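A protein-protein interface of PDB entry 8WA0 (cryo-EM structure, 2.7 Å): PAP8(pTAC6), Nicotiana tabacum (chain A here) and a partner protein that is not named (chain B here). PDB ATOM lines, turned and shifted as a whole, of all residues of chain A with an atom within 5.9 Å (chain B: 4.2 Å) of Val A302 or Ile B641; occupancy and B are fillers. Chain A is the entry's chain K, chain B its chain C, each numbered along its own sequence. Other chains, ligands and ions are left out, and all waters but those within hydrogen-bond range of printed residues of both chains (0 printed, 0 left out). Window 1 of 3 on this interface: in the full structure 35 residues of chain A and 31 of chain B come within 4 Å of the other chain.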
ATOM      1  N   ASP A 297      15.877 -28.916  13.968  1.00  0.00           N
ATOM      2  CA  ASP A 297      17.167 -28.785  13.347  1.00  0.00           C
ATOM      3  C   ASP A 297      18.002 -27.769  14.057  1.00  0.00           C
ATOM      4  O   ASP A 297      17.491 -26.758  14.506  1.00  0.00           O
ATOM      5  CB  ASP A 297      16.999 -28.399  11.897  1.00  0.00           C
ATOM      6  CG  ASP A 297      16.437 -29.518  11.055  1.00  0.00           C
ATOM      7  OD1 ASP A 297      16.319 -30.653  11.563  1.00  0.00           O
ATOM      8  OD2 ASP A 297      16.119 -29.264   9.875  1.00  0.00           O
ATOM      9  N   ASP A 298      19.288 -28.018  14.172  1.00  0.00           N
ATOM     10  CA  ASP A 298      20.201 -27.108  14.835  1.00  0.00           C
ATOM     11  C   ASP A 298      20.358 -25.865  14.047  1.00  0.00           C
ATOM     12  O   ASP A 298      20.104 -25.847  12.851  1.00  0.00           O
ATOM     13  CB  ASP A 298      21.552 -27.776  14.995  1.00  0.00           C
ATOM     14  CG  ASP A 298      22.091 -28.324  13.697  1.00  0.00           C
ATOM     15  OD1 ASP A 298      21.616 -29.392  13.255  1.00  0.00           O
ATOM     16  OD2 ASP A 298      23.000 -27.695  13.119  1.00  0.00           O
ATOM     17  N   PRO A 299      20.777 -24.803  14.689  1.00  0.00           N
ATOM     18  CA  PRO A 299      20.905 -23.533  14.009  1.00  0.00           C
ATOM     19  C   PRO A 299      21.833 -23.481  12.787  1.00  0.00           C
ATOM     20  O   PRO A 299      21.477 -22.817  11.837  1.00  0.00           O
ATOM     21  CB  PRO A 299      21.371 -22.654  15.130  1.00  0.00           C
ATOM     22  CG  PRO A 299      20.627 -23.147  16.298  1.00  0.00           C
ATOM     23  CD  PRO A 299      20.736 -24.629  16.148  1.00  0.00           C
ATOM     24  N   THR A 300      22.960 -24.151  12.771  1.00  0.00           N
ATOM     25  CA  THR A 300      23.822 -24.213  11.622  1.00  0.00           C
ATOM     26  C   THR A 300      23.191 -24.879  10.430  1.00  0.00           C
ATOM     27  O   THR A 300      23.344 -24.394   9.325  1.00  0.00           O
ATOM     28  CB  THR A 300      25.138 -24.884  11.984  1.00  0.00           C
ATOM     29  N   THR A 301      22.445 -25.951  10.619  1.00  0.00           N
ATOM     30  CA  THR A 301      21.789 -26.625   9.531  1.00  0.00           C
ATOM     31  C   THR A 301      20.783 -25.789   8.815  1.00  0.00           C
ATOM     32  O   THR A 301      20.727 -25.826   7.602  1.00  0.00           O
ATOM     33  CB  THR A 301      21.266 -27.990   9.915  1.00  0.00           C
ATOM     34  OG1 THR A 301      22.340 -28.776  10.426  1.00  0.00           O
ATOM     35  CG2 THR A 301      20.675 -28.712   8.734  1.00  0.00           C
ATOM     36  N   VAL A 302      20.031 -24.984   9.499  1.00  0.00           N
ATOM     37  CA  VAL A 302      19.125 -24.135   8.821  1.00  0.00           C
ATOM     38  C   VAL A 302      19.818 -23.135   7.919  1.00  0.00           C
ATOM     39  O   VAL A 302      19.408 -22.968   6.778  1.00  0.00           O
ATOM     40  CB  VAL A 302      18.080 -23.574   9.791  1.00  0.00           C
ATOM     41  CG1 VAL A 302      17.653 -24.673  10.736  1.00  0.00           C
ATOM     42  CG2 VAL A 302      18.632 -22.434  10.593  1.00  0.00           C
ATOM     43  N   ILE A 303      20.890 -22.515   8.358  1.00  0.00           N
ATOM     44  CA  ILE A 303      21.637 -21.592   7.537  1.00  0.00           C
ATOM     45  C   ILE A 303      22.311 -22.273   6.376  1.00  0.00           C
ATOM     46  O   ILE A 303      22.248 -21.804   5.252  1.00  0.00           O
ATOM     47  CB  ILE A 303      22.634 -20.790   8.386  1.00  0.00           C
ATOM     48  CG1 ILE A 303      21.930 -20.167   9.576  1.00  0.00           C
ATOM     49  CG2 ILE A 303      23.307 -19.714   7.555  1.00  0.00           C
ATOM     50  CD1 ILE A 303      22.876 -19.606  10.601  1.00  0.00           C
ATOM     51  N   GLU A 304      22.908 -23.407   6.622  1.00  0.00           N
ATOM     52  CA  GLU A 304      23.599 -24.132   5.601  1.00  0.00           C
ATOM     53  C   GLU A 304      22.723 -24.661   4.523  1.00  0.00           C
ATOM     54  O   GLU A 304      23.119 -24.671   3.371  1.00  0.00           O
ATOM     55  CB  GLU A 304      24.433 -25.177   6.243  1.00  0.00           C
ATOM     56  N   LYS A 305      21.530 -25.095   4.850  1.00  0.00           N
ATOM     57  CA  LYS A 305      20.612 -25.556   3.863  1.00  0.00           C
ATOM     58  C   LYS A 305      20.215 -24.500   2.927  1.00  0.00           C
ATOM     59  O   LYS A 305      20.112 -24.747   1.736  1.00  0.00           O
ATOM     60  CB  LYS A 305      19.416 -26.184   4.491  1.00  0.00           C
ATOM     61  CG  LYS A 305      19.622 -27.624   4.897  1.00  0.00           C
ATOM     62  CD  LYS A 305      18.398 -28.165   5.605  1.00  0.00           C
ATOM     63  CE  LYS A 305      17.129 -27.879   4.821  1.00  0.00           C
ATOM     64  NZ  LYS A 305      17.117 -28.525   3.480  1.00  0.00           N
ATOM     65  N   GLU A 306      20.000 -23.314   3.412  1.00  0.00           N
ATOM     66  CA  GLU A 306      19.628 -22.212   2.568  1.00  0.00           C
ATOM     67  C   GLU A 306      20.678 -21.755   1.628  1.00  0.00           C
ATOM     68  O   GLU A 306      20.402 -21.503   0.467  1.00  0.00           O
ATOM     69  CB  GLU A 306      19.091 -21.062   3.379  1.00  0.00           C
ATOM     70  CG  GLU A 306      18.400 -19.989   2.568  1.00  0.00           C
ATOM     71  CD  GLU A 306      17.506 -19.116   3.421  1.00  0.00           C
ATOM     72  OE1 GLU A 306      17.147 -19.554   4.533  1.00  0.00           O
ATOM     73  OE2 GLU A 306      17.157 -18.002   2.977  1.00  0.00           O
ATOM     74  N   GLU A 307      21.898 -21.677   2.091  1.00  0.00           N
ATOM     75  CA  GLU A 307      22.981 -21.291   1.260  1.00  0.00           C
ATOM     76  C   GLU A 307      23.204 -22.264   0.144  1.00  0.00           C
ATOM     77  O   GLU A 307      23.433 -21.851  -0.968  1.00  0.00           O
ATOM     78  CB  GLU A 307      24.207 -21.104   2.110  1.00  0.00           C
ATOM     79  CG  GLU A 307      24.116 -19.996   3.136  1.00  0.00           C
ATOM     80  CD  GLU A 307      24.116 -18.615   2.510  1.00  0.00           C
ATOM     81  OE1 GLU A 307      24.767 -18.430   1.460  1.00  0.00           O
ATOM     82  OE2 GLU A 307      23.472 -17.708   3.078  1.00  0.00           O
ATOM     83  N   PRO B 627      13.536 -13.306   9.743  1.00  0.00           N
ATOM     84  CA  PRO B 627      14.139 -14.554  10.146  1.00  0.00           C
ATOM     85  C   PRO B 627      13.924 -15.736   9.231  1.00  0.00           C
ATOM     86  O   PRO B 627      12.817 -15.882   8.729  1.00  0.00           O
ATOM     87  CB  PRO B 627      13.438 -14.807  11.443  1.00  0.00           C
ATOM     88  CG  PRO B 627      13.236 -13.486  12.036  1.00  0.00           C
ATOM     89  CD  PRO B 627      12.971 -12.577  10.885  1.00  0.00           C
ATOM     90  N   ILE B 628      14.929 -16.575   9.004  1.00  0.00           N
ATOM     91  CA  ILE B 628      14.747 -17.786   8.213  1.00  0.00           C
ATOM     92  C   ILE B 628      13.820 -18.772   8.857  1.00  0.00           C
ATOM     93  O   ILE B 628      12.966 -19.299   8.190  1.00  0.00           O
ATOM     94  CB  ILE B 628      16.064 -18.425   7.718  1.00  0.00           C
ATOM     95  CG1 ILE B 628      16.794 -19.200   8.805  1.00  0.00           C
ATOM     96  CG2 ILE B 628      16.999 -17.372   7.170  1.00  0.00           C
ATOM     97  CD1 ILE B 628      18.198 -19.582   8.401  1.00  0.00           C
ATOM     98  N   GLU B 629      13.943 -18.998  10.149  1.00  0.00           N
ATOM     99  CA  GLU B 629      13.092 -19.891  10.883  1.00  0.00           C
ATOM    100  C   GLU B 629      12.916 -19.388  12.278  1.00  0.00           C
ATOM    101  O   GLU B 629      13.879 -18.976  12.882  1.00  0.00           O
ATOM    102  CB  GLU B 629      13.730 -21.249  10.969  1.00  0.00           C
ATOM    103  CG  GLU B 629      13.673 -22.094   9.718  1.00  0.00           C
ATOM    104  CD  GLU B 629      14.163 -23.504   9.956  1.00  0.00           C
ATOM    105  OE1 GLU B 629      13.960 -24.362   9.072  1.00  0.00           O
ATOM    106  OE2 GLU B 629      14.745 -23.758  11.031  1.00  0.00           O
ATOM    107  N   TYR B 639      13.342 -19.070  19.703  1.00  0.00           N
ATOM    108  CA  TYR B 639      14.655 -18.935  19.110  1.00  0.00           C
ATOM    109  C   TYR B 639      14.467 -18.424  17.703  1.00  0.00           C
ATOM    110  O   TYR B 639      13.680 -18.973  16.976  1.00  0.00           O
ATOM    111  CB  TYR B 639      15.368 -20.275  19.089  1.00  0.00           C
ATOM    112  CG  TYR B 639      15.598 -20.971  20.388  1.00  0.00           C
ATOM    113  CD1 TYR B 639      14.600 -21.713  20.986  1.00  0.00           C
ATOM    114  CD2 TYR B 639      16.831 -20.935  20.991  1.00  0.00           C
ATOM    115  CE1 TYR B 639      14.816 -22.367  22.175  1.00  0.00           C
ATOM    116  CE2 TYR B 639      17.062 -21.588  22.180  1.00  0.00           C
ATOM    117  CZ  TYR B 639      16.050 -22.302  22.767  1.00  0.00           C
ATOM    118  OH  TYR B 639      16.281 -22.954  23.952  1.00  0.00           O
ATOM    119  N   GLU B 640      15.132 -17.351  17.324  1.00  0.00           N
ATOM    120  CA  GLU B 640      15.055 -16.791  15.993  1.00  0.00           C
ATOM    121  C   GLU B 640      16.331 -16.881  15.186  1.00  0.00           C
ATOM    122  O   GLU B 640      17.288 -16.242  15.526  1.00  0.00           O
ATOM    123  CB  GLU B 640      14.693 -15.350  16.101  1.00  0.00           C
ATOM    124  CG  GLU B 640      13.431 -15.058  16.875  1.00  0.00           C
ATOM    125  CD  GLU B 640      13.164 -13.575  16.977  1.00  0.00           C
ATOM    126  OE1 GLU B 640      14.051 -12.788  16.589  1.00  0.00           O
ATOM    127  OE2 GLU B 640      12.074 -13.192  17.446  1.00  0.00           O
ATOM    128  N   ILE B 641      16.341 -17.597  14.075  1.00  0.00           N
ATOM    129  CA  ILE B 641      17.536 -17.816  13.297  1.00  0.00           C
ATOM    130  C   ILE B 641      17.558 -16.956  12.091  1.00  0.00           C
ATOM    131  O   ILE B 641      16.671 -17.017  11.288  1.00  0.00           O
ATOM    132  CB  ILE B 641      17.700 -19.280  12.941  1.00  0.00           C
ATOM    133  CG1 ILE B 641      17.514 -20.150  14.174  1.00  0.00           C
ATOM    134  CG2 ILE B 641      19.036 -19.519  12.273  1.00  0.00           C
ATOM    135  CD1 ILE B 641      17.147 -21.577  13.862  1.00  0.00           C
ATOM    136  N   TYR B 642      18.488 -16.034  12.033  1.00  0.00           N
ATOM    137  CA  TYR B 642      18.632 -15.163  10.920  1.00  0.00           C
ATOM    138  C   TYR B 642      19.922 -15.657  10.399  1.00  0.00           C
ATOM    139  O   TYR B 642      20.553 -16.485  11.023  1.00  0.00           O
ATOM    140  CB  TYR B 642      18.810 -13.715  11.301  1.00  0.00           C
ATOM    141  CG  TYR B 642      17.744 -13.001  12.064  1.00  0.00           C
ATOM    142  CD1 TYR B 642      17.517 -13.265  13.390  1.00  0.00           C
ATOM    143  CD2 TYR B 642      17.036 -11.987  11.476  1.00  0.00           C
ATOM    144  CE1 TYR B 642      16.568 -12.575  14.094  1.00  0.00           C
ATOM    145  CE2 TYR B 642      16.090 -11.289  12.175  1.00  0.00           C
ATOM    146  CZ  TYR B 642      15.862 -11.592  13.481  1.00  0.00           C
ATOM    147  OH  TYR B 642      14.912 -10.900  14.177  1.00  0.00           O
ATOM    148  N   TYR B 645      22.879 -14.189  12.680  1.00  0.00           N
ATOM    149  CA  TYR B 645      22.611 -14.137  14.110  1.00  0.00           C
ATOM    150  C   TYR B 645      21.468 -14.956  14.733  1.00  0.00           C
ATOM    151  O   TYR B 645      20.498 -15.216  14.067  1.00  0.00           O
ATOM    152  CB  TYR B 645      22.566 -12.702  14.591  1.00  0.00           C
ATOM    153  CG  TYR B 645      21.839 -11.656  13.816  1.00  0.00           C
ATOM    154  CD1 TYR B 645      22.493 -10.885  12.878  1.00  0.00           C
ATOM    155  CD2 TYR B 645      20.527 -11.358  14.099  1.00  0.00           C
ATOM    156  CE1 TYR B 645      21.835  -9.899  12.182  1.00  0.00           C
ATOM    157  CE2 TYR B 645      19.859 -10.369  13.416  1.00  0.00           C
ATOM    158  CZ  TYR B 645      20.516  -9.644  12.457  1.00  0.00           C
ATOM    159  OH  TYR B 645      19.852  -8.655  11.774  1.00  0.00           O
ATOM    160  N   LEU B 646      21.577 -15.367  16.001  1.00  0.00           N
ATOM    161  CA  LEU B 646      20.517 -16.094  16.732  1.00  0.00           C
ATOM    162  C   LEU B 646      20.118 -15.298  17.945  1.00  0.00           C
ATOM    163  O   LEU B 646      20.948 -15.056  18.797  1.00  0.00           O
ATOM    164  CB  LEU B 646      20.999 -17.473  17.188  1.00  0.00           C
ATOM    165  CG  LEU B 646      20.211 -18.402  18.079  1.00  0.00           C
ATOM    166  CD1 LEU B 646      18.947 -18.872  17.388  1.00  0.00           C
ATOM    167  CD2 LEU B 646      21.114 -19.574  18.394  1.00  0.00           C
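Among the printed residues, merely in contact across the chains: Val A302 with Ile B628, Val A302 with Glu B629, Val A302 with Ile B641, Ile A303 with Ile B628, Ile A303 with Tyr B642 and Glu A306 with Ile B628.
Val A302 touches just these residues of chain B: Ile B628, Glu B629 and Ile B641.
Of the printed residues of chain A, Ile B641 touches Val A302 (3.4 Å).
Printed residues of chain B within 4 Å of Ile A303: Ile B628 (3.96 Å) and Tyr B642 (3.9 Å).
Of the printed residues of chain A, Glu B629 touches Val A302.
Tyr B639 touches none of the printed residues of chain A.
Asp A297 touches none of the printed residues of chain B.
The nearest printed residue of chain B that does not touch Val A302 is Tyr B642 (6.3 Å).
The nearest printed residue of chain A that does not touch Ile B641 is Ile A303 (4.01 Å).
The nearest printed residue of chain A that does not touch Tyr B642 is Val A302 (6.3 Å).
O of Ile B641 lies within hydrogen-bond range of N of Ile B628 (2.9 Å).
The backbone carbonyl oxygen (O) of Glu B629 sits at hydrogen-bond distance from the backbone NH (N) of Ile B641 (3.1 Å).
The side-chain carboxylate (OE1) of Glu B640 is in hydrogen-bond range of the side-chain hydroxyl (OH) of Tyr B642.
Of the 11 printed residues of chain A, 3 touch a printed residue of chain B.
Hydrophobic or aromatic side chains of chain A that line the printed part of chain B: Val A302 and Ile A303.
Of the 9 printed residues of chain B, 4 touch a printed residue of chain A.
Hydrophobic or aromatic side chains of chain B within 4 Å of the printed part of chain A: Ile B628 and Ile B641.
Among the printed residues, 6 pairs touch across the chains.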
